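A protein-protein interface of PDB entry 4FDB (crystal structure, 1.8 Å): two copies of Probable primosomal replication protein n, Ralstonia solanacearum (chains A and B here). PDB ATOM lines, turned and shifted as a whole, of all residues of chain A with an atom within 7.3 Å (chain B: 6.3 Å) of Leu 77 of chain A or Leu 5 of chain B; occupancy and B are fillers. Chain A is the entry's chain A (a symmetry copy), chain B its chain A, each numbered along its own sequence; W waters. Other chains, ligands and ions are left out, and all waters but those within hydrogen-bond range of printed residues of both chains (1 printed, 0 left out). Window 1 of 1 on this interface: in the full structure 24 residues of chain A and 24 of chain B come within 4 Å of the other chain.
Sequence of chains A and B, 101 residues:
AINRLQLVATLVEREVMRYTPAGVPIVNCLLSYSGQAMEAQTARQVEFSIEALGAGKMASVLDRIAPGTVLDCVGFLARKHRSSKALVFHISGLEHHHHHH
Printed residues of chain A that touch a printed residue of chain B: Ile 2, Asn 3, Arg 4, Leu 5, Gln 6, Ile 50, Phe 76, Leu 77, Arg 79 and Leu 87.
Of the 15 printed residues of chain B, 10 touch a printed residue of chain A.
Hydrophobic or aromatic side chains of chain B within 4 Å of the printed part of chain A: Leu 5, Leu 7, Tyr 33, Val 46, Phe 48, Ile 50 and Leu 77.
Among the printed residues, merely in contact across the chains: Ile 2 of chain A with Gln 6 of chain B, Ile 2 of chain A with Leu 7 of chain B, Ile 2 of chain A with Tyr 33 of chain B, Asn 3 of chain A with Gln 6 of chain B, Asn 3 of chain A with Leu 7 of chain B, Asn 3 of chain A with Tyr 33 of chain B, Asn 3 of chain A with Val 46 of chain B, Asn 3 of chain A with Phe 48 of chain B, Arg 4 of chain A with Arg 4 of chain B, Arg 4 of chain A with Leu 5 of chain B, Leu 5 of chain A with Arg 4 of chain B, Leu 5 of chain A with Leu 77 of chain B, Gln 6 of chain A with Asn 3 of chain B, Ile 50 of chain A with Leu 77 of chain B, Phe 76 of chain A with Val 46 of chain B, Leu 77 of chain A with Leu 5 of chain B, Leu 77 of chain A with Val 46 of chain B, Leu 77 of chain A with Phe 48 of chain B, Leu 77 of chain A with Ile 50 of chain B, Arg 79 of chain A with Phe 48 of chain B and Leu 87 of chain A with Phe 48 of chain B.
Water W1 bridges OH of Tyr 33 of chain B (2.9 Å) and ND2 of Asn 3 of chain A (3.0 Å).
The backbone carbonyl oxygen (O) of Arg 4 of chain B lies within hydrogen-bond range of the backbone NH (N) of Gln 6 of chain A (2.9 Å).
The backbone NH (N) of Gln 6 of chain B lies within hydrogen-bond range of the backbone carbonyl oxygen (O) of Arg 4 of chain A.
The side-chain amide nitrogen of Asn 3 of chain B sits at hydrogen-bond distance from the backbone carbonyl oxygen of Leu 77 of chain B (2.8 Å).
The backbone NH of Leu 5 of chain B is in hydrogen-bond range of the backbone carbonyl oxygen of Gly 75 of chain B.
The backbone carbonyl oxygen (O) of Leu 7 of chain B sits at hydrogen-bond distance from the backbone NH (N) of Cys 73 of chain B, at 2.8 Å.
The backbone carbonyl oxygen (O) of Phe 48 of chain B lies within hydrogen-bond range of the backbone NH (N) of Tyr 33 of chain B, 2.7 Å away.
The side-chain amide nitrogen of Asn 3 of chain A sits at hydrogen-bond distance from the backbone carbonyl oxygen of Leu 77 of chain A, 2.8 Å away.
The backbone NH of Leu 5 of chain A is in hydrogen-bond range of the backbone carbonyl oxygen of Gly 75 of chain A.
Of chain B, only Leu 5 (3.97 Å), Val 46 (3.5 Å), Phe 48 (3.3 Å) and Ile 50 (3.9 Å) come within 4 Å of Leu 77 of chain A.
Of the printed residues of chain B, Arg 79 of chain A touches Phe 48 (3.7 Å).
Of the printed residues of chain B, Leu 87 of chain A touches Phe 48.
Val 88 of chain A touches none of the printed residues of chain B.
Of chain A, only Arg 4 and Leu 77 come within 4 Å of Leu 5 of chain B.
The nearest residue of chain A that does not touch Leu 5 of chain B is Leu 5 of chain A (4.1 Å).
The nearest printed residue of chain B that does not touch Ile 50 of chain A is Asn 3 of chain B (7.8 Å).
Asn 3 of chain A touches Gln 6 of chain B, and with the chains exchanged Gln 6 of chain A touches Asn 3 of chain B.
Arg 4 of chain A touches its own counterpart, Arg 4 of chain B.
Arg 4 of chain A touches Leu 5 of chain B, and with the chains exchanged Leu 5 of chain A touches Arg 4 of chain B.
Ile 50 of chain A touches Leu 77 of chain B, and with the chains exchanged Leu 77 of chain A touches Ile 50 of chain B.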
ATOM      1  N   ILE A   2     -29.742  -0.125  12.670  1.00  0.00           N
ATOM      2  CA  ILE A   2     -29.146  -0.977  11.645  1.00  0.00           C
ATOM      3  C   ILE A   2     -28.965  -0.226  10.328  1.00  0.00           C
ATOM      4  O   ILE A   2     -29.779   0.597   9.941  1.00  0.00           O
ATOM      5  CB  ILE A   2     -29.912  -2.307  11.422  1.00  0.00           C
ATOM      6  CG1 ILE A   2     -29.035  -3.300  10.645  1.00  0.00           C
ATOM      7  CG2 ILE A   2     -31.204  -2.073  10.675  1.00  0.00           C
ATOM      8  CD1 ILE A   2     -29.655  -4.669  10.470  1.00  0.00           C
ATOM      9  N   ASN A   3     -27.846  -0.504   9.669  1.00  0.00           N
ATOM     10  CA  ASN A   3     -27.528   0.048   8.355  1.00  0.00           C
ATOM     11  C   ASN A   3     -26.622  -1.006   7.779  1.00  0.00           C
ATOM     12  O   ASN A   3     -25.422  -1.003   8.043  1.00  0.00           O
ATOM     13  CB  ASN A   3     -26.814   1.399   8.512  1.00  0.00           C
ATOM     14  CG  ASN A   3     -26.104   1.878   7.230  1.00  0.00           C
ATOM     15  OD1 ASN A   3     -26.267   1.327   6.135  1.00  0.00           O
ATOM     16  ND2 ASN A   3     -25.279   2.905   7.389  1.00  0.00           N
ATOM     17  N   ARG A   4     -27.207  -1.932   7.020  1.00  0.00           N
ATOM     18  CA  ARG A   4     -26.441  -3.083   6.521  1.00  0.00           C
ATOM     19  C   ARG A   4     -26.877  -3.453   5.122  1.00  0.00           C
ATOM     20  O   ARG A   4     -28.044  -3.764   4.897  1.00  0.00           O
ATOM     21  CB  ARG A   4     -26.651  -4.283   7.454  1.00  0.00           C
ATOM     22  CG  ARG A   4     -25.890  -5.544   7.053  1.00  0.00           C
ATOM     23  CD  ARG A   4     -25.877  -6.560   8.190  1.00  0.00           C
ATOM     24  NE  ARG A   4     -25.081  -7.740   7.863  1.00  0.00           N
ATOM     25  CZ  ARG A   4     -25.591  -8.933   7.563  1.00  0.00           C
ATOM     26  NH1 ARG A   4     -24.785  -9.947   7.274  1.00  0.00           N
ATOM     27  NH2 ARG A   4     -26.906  -9.114   7.560  1.00  0.00           N
ATOM     28  N   LEU A   5     -25.929  -3.421   4.190  1.00  0.00           N
ATOM     29  CA  LEU A   5     -26.178  -3.793   2.811  1.00  0.00           C
ATOM     30  C   LEU A   5     -25.436  -5.096   2.529  1.00  0.00           C
ATOM     31  O   LEU A   5     -24.260  -5.224   2.869  1.00  0.00           O
ATOM     32  CB  LEU A   5     -25.655  -2.709   1.862  1.00  0.00           C
ATOM     33  CG  LEU A   5     -25.790  -3.064   0.368  1.00  0.00           C
ATOM     34  CD1 LEU A   5     -27.262  -3.217  -0.004  1.00  0.00           C
ATOM     35  CD2 LEU A   5     -25.134  -2.030  -0.542  1.00  0.00           C
ATOM     36  N   GLN A   6     -26.137  -6.062   1.945  1.00  0.00           N
ATOM     37  CA  GLN A   6     -25.507  -7.281   1.434  1.00  0.00           C
ATOM     38  C   GLN A   6     -25.662  -7.241  -0.068  1.00  0.00           C
ATOM     39  O   GLN A   6     -26.756  -7.039  -0.567  1.00  0.00           O
ATOM     40  CB  GLN A   6     -26.232  -8.511   1.954  1.00  0.00           C
ATOM     41  CG  GLN A   6     -26.260  -8.665   3.460  1.00  0.00           C
ATOM     42  CD  GLN A   6     -27.256  -9.717   3.884  1.00  0.00           C
ATOM     43  OE1 GLN A   6     -28.422  -9.418   4.144  1.00  0.00           O
ATOM     44  NE2 GLN A   6     -26.807 -10.968   3.934  1.00  0.00           N
ATOM     45  N   ILE A  50     -22.631   0.829  -8.263  1.00  0.00           N
ATOM     46  CA  ILE A  50     -22.575   1.570  -7.003  1.00  0.00           C
ATOM     47  C   ILE A  50     -21.122   1.826  -6.614  1.00  0.00           C
ATOM     48  O   ILE A  50     -20.260   0.960  -6.773  1.00  0.00           O
ATOM     49  CB  ILE A  50     -23.342   0.819  -5.895  1.00  0.00           C
ATOM     50  CG1 ILE A  50     -23.474   1.681  -4.636  1.00  0.00           C
ATOM     51  CG2 ILE A  50     -22.689  -0.543  -5.611  1.00  0.00           C
ATOM     52  CD1 ILE A  50     -24.342   1.029  -3.546  1.00  0.00           C
ATOM     53  N   GLU A  51     -20.836   3.045  -6.156  1.00  0.00           N
ATOM     54  CA  GLU A  51     -19.509   3.349  -5.648  1.00  0.00           C
ATOM     55  C   GLU A  51     -19.319   2.689  -4.295  1.00  0.00           C
ATOM     56  O   GLU A  51     -20.210   2.728  -3.447  1.00  0.00           O
ATOM     57  CB  GLU A  51     -19.326   4.869  -5.529  1.00  0.00           C
ATOM     58  CG  GLU A  51     -19.279   5.585  -6.881  1.00  0.00           C
ATOM     59  CD  GLU A  51     -17.936   5.434  -7.594  1.00  0.00           C
ATOM     60  OE1 GLU A  51     -16.978   4.922  -6.970  1.00  0.00           O
ATOM     61  OE2 GLU A  51     -17.835   5.829  -8.780  1.00  0.00           O
ATOM     62  N   GLY A  75     -21.664  -4.661   4.278  1.00  0.00           N
ATOM     63  CA  GLY A  75     -21.147  -3.425   4.815  1.00  0.00           C
ATOM     64  C   GLY A  75     -22.264  -2.468   5.070  1.00  0.00           C
ATOM     65  O   GLY A  75     -23.388  -2.897   5.362  1.00  0.00           O
ATOM     66  N   PHE A  76     -21.958  -1.180   4.969  1.00  0.00           N
ATOM     67  CA  PHE A  76     -22.944  -0.158   5.315  1.00  0.00           C
ATOM     68  C   PHE A  76     -22.886   1.009   4.354  1.00  0.00           C
ATOM     69  O   PHE A  76     -21.902   1.189   3.660  1.00  0.00           O
ATOM     70  CB  PHE A  76     -22.734   0.327   6.754  1.00  0.00           C
ATOM     71  CG  PHE A  76     -21.383   0.965   7.011  1.00  0.00           C
ATOM     72  CD1 PHE A  76     -21.227   2.346   6.960  1.00  0.00           C
ATOM     73  CD2 PHE A  76     -20.283   0.183   7.348  1.00  0.00           C
ATOM     74  CE1 PHE A  76     -19.991   2.941   7.232  1.00  0.00           C
ATOM     75  CE2 PHE A  76     -19.043   0.764   7.611  1.00  0.00           C
ATOM     76  CZ  PHE A  76     -18.892   2.137   7.537  1.00  0.00           C
ATOM     77  N   LEU A  77     -23.969   1.781   4.282  1.00  0.00           N
ATOM     78  CA  LEU A  77     -23.977   2.971   3.439  1.00  0.00           C
ATOM     79  C   LEU A  77     -23.538   4.195   4.242  1.00  0.00           C
ATOM     80  O   LEU A  77     -23.785   4.279   5.436  1.00  0.00           O
ATOM     81  CB  LEU A  77     -25.383   3.236   2.901  1.00  0.00           C
ATOM     82  CG  LEU A  77     -25.914   2.165   1.953  1.00  0.00           C
ATOM     83  CD1 LEU A  77     -27.346   2.519   1.540  1.00  0.00           C
ATOM     84  CD2 LEU A  77     -25.016   2.044   0.732  1.00  0.00           C
ATOM     85  N   ALA A  78     -22.911   5.154   3.567  1.00  0.00           N
ATOM     86  CA  ALA A  78     -22.534   6.407   4.198  1.00  0.00           C
ATOM     87  C   ALA A  78     -22.457   7.492   3.146  1.00  0.00           C
ATOM     88  O   ALA A  78     -22.551   7.202   1.963  1.00  0.00           O
ATOM     89  CB  ALA A  78     -21.215   6.272   4.936  1.00  0.00           C
ATOM     90  N   ARG A  79     -22.353   8.741   3.594  1.00  0.00           N
ATOM     91  CA  ARG A  79     -22.161   9.867   2.694  1.00  0.00           C
ATOM     92  C   ARG A  79     -20.735   9.868   2.177  1.00  0.00           C
ATOM     93  O   ARG A  79     -19.799   9.567   2.924  1.00  0.00           O
ATOM     94  CB  ARG A  79     -22.416  11.186   3.418  1.00  0.00           C
ATOM     95  CG  ARG A  79     -23.849  11.644   3.418  1.00  0.00           C
ATOM     96  CD  ARG A  79     -23.952  13.066   3.964  1.00  0.00           C
ATOM     97  NE  ARG A  79     -25.334  13.533   4.007  1.00  0.00           N
ATOM     98  CZ  ARG A  79     -25.890  14.112   5.066  1.00  0.00           C
ATOM     99  NH1 ARG A  79     -25.175  14.296   6.170  1.00  0.00           N
ATOM    100  NH2 ARG A  79     -27.158  14.506   5.024  1.00  0.00           N
ATOM    101  N   LEU A  87     -23.876   8.796  -2.069  1.00  0.00           N
ATOM    102  CA  LEU A  87     -23.599   7.759  -1.082  1.00  0.00           C
ATOM    103  C   LEU A  87     -22.521   6.799  -1.569  1.00  0.00           C
ATOM    104  O   LEU A  87     -22.294   6.647  -2.759  1.00  0.00           O
ATOM    105  CB  LEU A  87     -24.858   6.956  -0.760  1.00  0.00           C
ATOM    106  CG  LEU A  87     -26.041   7.704  -0.148  1.00  0.00           C
ATOM    107  CD1 LEU A  87     -27.103   6.682   0.234  1.00  0.00           C
ATOM    108  CD2 LEU A  87     -25.595   8.522   1.057  1.00  0.00           C
ATOM    109  N   VAL A  88     -21.883   6.137  -0.619  1.00  0.00           N
ATOM    110  CA  VAL A  88     -20.855   5.169  -0.926  1.00  0.00           C
ATOM    111  C   VAL A  88     -21.102   3.928  -0.078  1.00  0.00           C
ATOM    112  O   VAL A  88     -21.505   4.038   1.080  1.00  0.00           O
ATOM    113  CB  VAL A  88     -19.454   5.764  -0.663  1.00  0.00           C
ATOM    114  CG1 VAL A  88     -19.325   6.251   0.779  1.00  0.00           C
ATOM    115  CG2 VAL A  88     -18.366   4.755  -0.985  1.00  0.00           C
ATOM    116  N   PHE A  89     -20.878   2.755  -0.664  1.00  0.00           N
ATOM    117  CA  PHE A  89     -20.988   1.478   0.037  1.00  0.00           C
ATOM    118  C   PHE A  89     -19.657   1.150   0.726  1.00  0.00           C
ATOM    119  O   PHE A  89     -18.682   0.805   0.063  1.00  0.00           O
ATOM    120  CB  PHE A  89     -21.367   0.404  -0.993  1.00  0.00           C
ATOM    121  CG  PHE A  89     -21.462  -1.013  -0.448  1.00  0.00           C
ATOM    122  CD1 PHE A  89     -21.724  -1.271   0.891  1.00  0.00           C
ATOM    123  CD2 PHE A  89     -21.313  -2.092  -1.313  1.00  0.00           C
ATOM    124  CE1 PHE A  89     -21.818  -2.584   1.361  1.00  0.00           C
ATOM    125  CE2 PHE A  89     -21.394  -3.403  -0.856  1.00  0.00           C
ATOM    126  CZ  PHE A  89     -21.652  -3.652   0.486  1.00  0.00           C
ATOM    127  N   HIS A  90     -19.612   1.269   2.051  1.00  0.00           N
ATOM    128  CA  HIS A  90     -18.411   0.882   2.796  1.00  0.00           C
ATOM    129  C   HIS A  90     -18.424  -0.620   3.018  1.00  0.00           C
ATOM    130  O   HIS A  90     -19.303  -1.148   3.689  1.00  0.00           O
ATOM    131  CB  HIS A  90     -18.358   1.579   4.159  1.00  0.00           C
ATOM    132  CG  HIS A  90     -18.007   3.030   4.093  1.00  0.00           C
ATOM    133  ND1 HIS A  90     -16.897   3.554   4.723  1.00  0.00           N
ATOM    134  CD2 HIS A  90     -18.639   4.078   3.513  1.00  0.00           C
ATOM    135  CE1 HIS A  90     -16.850   4.857   4.519  1.00  0.00           C
ATOM    136  NE2 HIS A  90     -17.900   5.203   3.793  1.00  0.00           N
ATOM    137  N   ASN B   3     -29.157  -8.717  -2.935  1.00  0.00           N
ATOM    138  CA  ASN B   3     -29.185  -7.258  -2.962  1.00  0.00           C
ATOM    139  C   ASN B   3     -30.197  -6.939  -1.895  1.00  0.00           C
ATOM    140  O   ASN B   3     -31.397  -6.941  -2.160  1.00  0.00           O
ATOM    141  CB  ASN B   3     -29.632  -6.767  -4.347  1.00  0.00           C
ATOM    142  CG  ASN B   3     -30.059  -5.285  -4.372  1.00  0.00           C
ATOM    143  OD1 ASN B   3     -29.865  -4.522  -3.418  1.00  0.00           O
ATOM    144  ND2 ASN B   3     -30.678  -4.892  -5.478  1.00  0.00           N
ATOM    145  N   ARG B   4     -29.712  -6.701  -0.677  1.00  0.00           N
ATOM    146  CA  ARG B   4     -30.617  -6.517   0.465  1.00  0.00           C
ATOM    147  C   ARG B   4     -30.082  -5.464   1.410  1.00  0.00           C
ATOM    148  O   ARG B   4     -28.980  -5.603   1.935  1.00  0.00           O
ATOM    149  CB  ARG B   4     -30.773  -7.844   1.218  1.00  0.00           C
ATOM    150  CG  ARG B   4     -31.708  -7.790   2.423  1.00  0.00           C
ATOM    151  CD  ARG B   4     -32.071  -9.192   2.898  1.00  0.00           C
ATOM    152  NE  ARG B   4     -33.034  -9.168   3.996  1.00  0.00           N
ATOM    153  CZ  ARG B   4     -32.735  -9.431   5.266  1.00  0.00           C
ATOM    154  NH1 ARG B   4     -33.679  -9.380   6.197  1.00  0.00           N
ATOM    155  NH2 ARG B   4     -31.492  -9.754   5.606  1.00  0.00           N
ATOM    156  N   LEU B   5     -30.874  -4.417   1.623  1.00  0.00           N
ATOM    157  CA  LEU B   5     -30.524  -3.347   2.536  1.00  0.00           C
ATOM    158  C   LEU B   5     -31.465  -3.421   3.735  1.00  0.00           C
ATOM    159  O   LEU B   5     -32.678  -3.544   3.563  1.00  0.00           O
ATOM    160  CB  LEU B   5     -30.694  -1.986   1.854  1.00  0.00           C
ATOM    161  CG  LEU B   5     -30.436  -0.782   2.783  1.00  0.00           C
ATOM    162  CD1 LEU B   5     -28.988  -0.790   3.262  1.00  0.00           C
ATOM    163  CD2 LEU B   5     -30.749   0.553   2.113  1.00  0.00           C
ATOM    164  N   GLN B   6     -30.898  -3.380   4.936  1.00  0.00           N
ATOM    165  CA  GLN B   6     -31.683  -3.235   6.163  1.00  0.00           C
ATOM    166  C   GLN B   6     -31.328  -1.884   6.738  1.00  0.00           C
ATOM    167  O   GLN B   6     -30.159  -1.572   6.895  1.00  0.00           O
ATOM    168  CB  GLN B   6     -31.291  -4.300   7.174  1.00  0.00           C
ATOM    169  CG  GLN B   6     -31.492  -5.732   6.724  1.00  0.00           C
ATOM    170  CD  GLN B   6     -30.787  -6.698   7.646  1.00  0.00           C
ATOM    171  OE1 GLN B   6     -29.630  -7.056   7.425  1.00  0.00           O
ATOM    172  NE2 GLN B   6     -31.477  -7.112   8.706  1.00  0.00           N
ATOM    173  N   LEU B   7     -32.332  -1.079   7.061  1.00  0.00           N
ATOM    174  CA  LEU B   7     -32.059   0.272   7.489  1.00  0.00           C
ATOM    175  C   LEU B   7     -33.114   0.676   8.500  1.00  0.00           C
ATOM    176  O   LEU B   7     -34.300   0.482   8.260  1.00  0.00           O
ATOM    177  CB  LEU B   7     -32.089   1.216   6.286  1.00  0.00           C
ATOM    178  CG  LEU B   7     -31.496   2.618   6.513  1.00  0.00           C
ATOM    179  CD1 LEU B   7     -29.995   2.518   6.754  1.00  0.00           C
ATOM    180  CD2 LEU B   7     -31.763   3.514   5.326  1.00  0.00           C
ATOM    181  N   TYR B  33     -31.066   8.546   7.918  1.00  0.00           N
ATOM    182  CA  TYR B  33     -30.373   7.642   8.814  1.00  0.00           C
ATOM    183  C   TYR B  33     -29.396   8.395   9.710  1.00  0.00           C
ATOM    184  O   TYR B  33     -28.636   9.259   9.253  1.00  0.00           O
ATOM    185  CB  TYR B  33     -29.603   6.550   8.028  1.00  0.00           C
ATOM    186  CG  TYR B  33     -28.798   5.666   8.962  1.00  0.00           C
ATOM    187  CD1 TYR B  33     -29.370   4.554   9.563  1.00  0.00           C
ATOM    188  CD2 TYR B  33     -27.476   5.980   9.287  1.00  0.00           C
ATOM    189  CE1 TYR B  33     -28.643   3.775  10.456  1.00  0.00           C
ATOM    190  CE2 TYR B  33     -26.750   5.200  10.165  1.00  0.00           C
ATOM    191  CZ  TYR B  33     -27.345   4.108  10.753  1.00  0.00           C
ATOM    192  OH  TYR B  33     -26.613   3.344  11.635  1.00  0.00           O
ATOM    193  N   VAL B  46     -22.406   7.821  11.495  1.00  0.00           N
ATOM    194  CA  VAL B  46     -22.814   7.841  10.102  1.00  0.00           C
ATOM    195  C   VAL B  46     -24.145   8.560  10.038  1.00  0.00           C
ATOM    196  O   VAL B  46     -25.040   8.268  10.829  1.00  0.00           O
ATOM    197  CB  VAL B  46     -22.971   6.409   9.547  1.00  0.00           C
ATOM    198  CG1 VAL B  46     -23.603   6.431   8.150  1.00  0.00           C
ATOM    199  CG2 VAL B  46     -21.619   5.698   9.519  1.00  0.00           C
ATOM    200  N   PHE B  48     -26.874  10.067   6.873  1.00  0.00           N
ATOM    201  CA  PHE B  48     -27.177  10.362   5.481  1.00  0.00           C
ATOM    202  C   PHE B  48     -28.677  10.312   5.273  1.00  0.00           C
ATOM    203  O   PHE B  48     -29.424   9.814   6.127  1.00  0.00           O
ATOM    204  CB  PHE B  48     -26.469   9.359   4.535  1.00  0.00           C
ATOM    205  CG  PHE B  48     -26.907   7.929   4.712  1.00  0.00           C
ATOM    206  CD1 PHE B  48     -27.949   7.404   3.948  1.00  0.00           C
ATOM    207  CD2 PHE B  48     -26.262   7.101   5.618  1.00  0.00           C
ATOM    208  CE1 PHE B  48     -28.357   6.086   4.105  1.00  0.00           C
ATOM    209  CE2 PHE B  48     -26.673   5.785   5.781  1.00  0.00           C
ATOM    210  CZ  PHE B  48     -27.707   5.275   5.021  1.00  0.00           C
ATOM    211  N   ILE B  50     -31.601   9.115   2.220  1.00  0.00           N
ATOM    212  CA  ILE B  50     -31.675   8.250   1.042  1.00  0.00           C
ATOM    213  C   ILE B  50     -33.088   8.276   0.466  1.00  0.00           C
ATOM    214  O   ILE B  50     -34.075   8.275   1.203  1.00  0.00           O
ATOM    215  CB  ILE B  50     -31.224   6.816   1.391  1.00  0.00           C
ATOM    216  CG1 ILE B  50     -31.092   5.959   0.129  1.00  0.00           C
ATOM    217  CG2 ILE B  50     -32.164   6.190   2.432  1.00  0.00           C
ATOM    218  CD1 ILE B  50     -30.520   4.558   0.408  1.00  0.00           C
ATOM    219  N   CYS B  73     -36.733  -0.809   8.082  1.00  0.00           N
ATOM    220  CA  CYS B  73     -36.993  -1.120   6.678  1.00  0.00           C
ATOM    221  C   CYS B  73     -36.093  -2.222   6.160  1.00  0.00           C
ATOM    222  O   CYS B  73     -34.923  -2.313   6.542  1.00  0.00           O
ATOM    223  CB  CYS B  73     -36.709   0.101   5.809  1.00  0.00           C
ATOM    224  SG  CYS B  73     -37.547   1.602   6.349  1.00  0.00           S
ATOM    225  N   VAL B  74     -36.648  -3.061   5.297  1.00  0.00           N
ATOM    226  CA  VAL B  74     -35.825  -3.963   4.502  1.00  0.00           C
ATOM    227  C   VAL B  74     -36.195  -3.777   3.041  1.00  0.00           C
ATOM    228  O   VAL B  74     -37.289  -3.320   2.707  1.00  0.00           O
ATOM    229  CB  VAL B  74     -35.988  -5.433   4.917  1.00  0.00           C
ATOM    230  CG1 VAL B  74     -35.333  -5.683   6.271  1.00  0.00           C
ATOM    231  CG2 VAL B  74     -37.456  -5.832   4.937  1.00  0.00           C
ATOM    232  N   GLY B  75     -35.274  -4.109   2.155  1.00  0.00           N
ATOM    233  CA  GLY B  75     -35.603  -4.044   0.751  1.00  0.00           C
ATOM    234  C   GLY B  75     -34.362  -4.148  -0.073  1.00  0.00           C
ATOM    235  O   GLY B  75     -33.393  -4.791   0.351  1.00  0.00           O
ATOM    236  N   PHE B  76     -34.393  -3.525  -1.246  1.00  0.00           N
ATOM    237  CA  PHE B  76     -33.279  -3.662  -2.182  1.00  0.00           C
ATOM    238  C   PHE B  76     -32.978  -2.351  -2.873  1.00  0.00           C
ATOM    239  O   PHE B  76     -33.807  -1.459  -2.894  1.00  0.00           O
ATOM    240  CB  PHE B  76     -33.576  -4.753  -3.217  1.00  0.00           C
ATOM    241  CG  PHE B  76     -34.797  -4.487  -4.076  1.00  0.00           C
ATOM    242  CD1 PHE B  76     -34.668  -3.907  -5.334  1.00  0.00           C
ATOM    243  CD2 PHE B  76     -36.063  -4.862  -3.641  1.00  0.00           C
ATOM    244  CE1 PHE B  76     -35.788  -3.693  -6.145  1.00  0.00           C
ATOM    245  CE2 PHE B  76     -37.188  -4.645  -4.438  1.00  0.00           C
ATOM    246  CZ  PHE B  76     -37.054  -4.047  -5.678  1.00  0.00           C
ATOM    247  N   LEU B  77     -31.764  -2.216  -3.405  1.00  0.00           N
ATOM    248  CA  LEU B  77     -31.410  -1.017  -4.155  1.00  0.00           C
ATOM    249  C   LEU B  77     -31.702  -1.214  -5.643  1.00  0.00           C
ATOM    250  O   LEU B  77     -31.602  -2.319  -6.156  1.00  0.00           O
ATOM    251  CB  LEU B  77     -29.922  -0.709  -4.000  1.00  0.00           C
ATOM    252  CG  LEU B  77     -29.492  -0.341  -2.582  1.00  0.00           C
ATOM    253  CD1 LEU B  77     -27.977  -0.119  -2.553  1.00  0.00           C
ATOM    254  CD2 LEU B  77     -30.228   0.903  -2.110  1.00  0.00           C
ATOM    255  N   PHE B  89     -33.924   3.249  -2.752  1.00  0.00           N
ATOM    256  CA  PHE B  89     -34.161   2.124  -1.852  1.00  0.00           C
ATOM    257  C   PHE B  89     -35.610   1.640  -1.999  1.00  0.00           C
ATOM    258  O   PHE B  89     -36.538   2.310  -1.553  1.00  0.00           O
ATOM    259  CB  PHE B  89     -33.869   2.594  -0.420  1.00  0.00           C
ATOM    260  CG  PHE B  89     -34.129   1.562   0.668  1.00  0.00           C
ATOM    261  CD1 PHE B  89     -34.102   0.198   0.411  1.00  0.00           C
ATOM    262  CD2 PHE B  89     -34.373   1.985   1.971  1.00  0.00           C
ATOM    263  CE1 PHE B  89     -34.331  -0.727   1.433  1.00  0.00           C
ATOM    264  CE2 PHE B  89     -34.613   1.075   2.994  1.00  0.00           C
ATOM    265  CZ  PHE B  89     -34.587  -0.287   2.728  1.00  0.00           C
HETATM  266  O   HOH W   1     -24.167   3.013  10.187  1.00  0.00           O
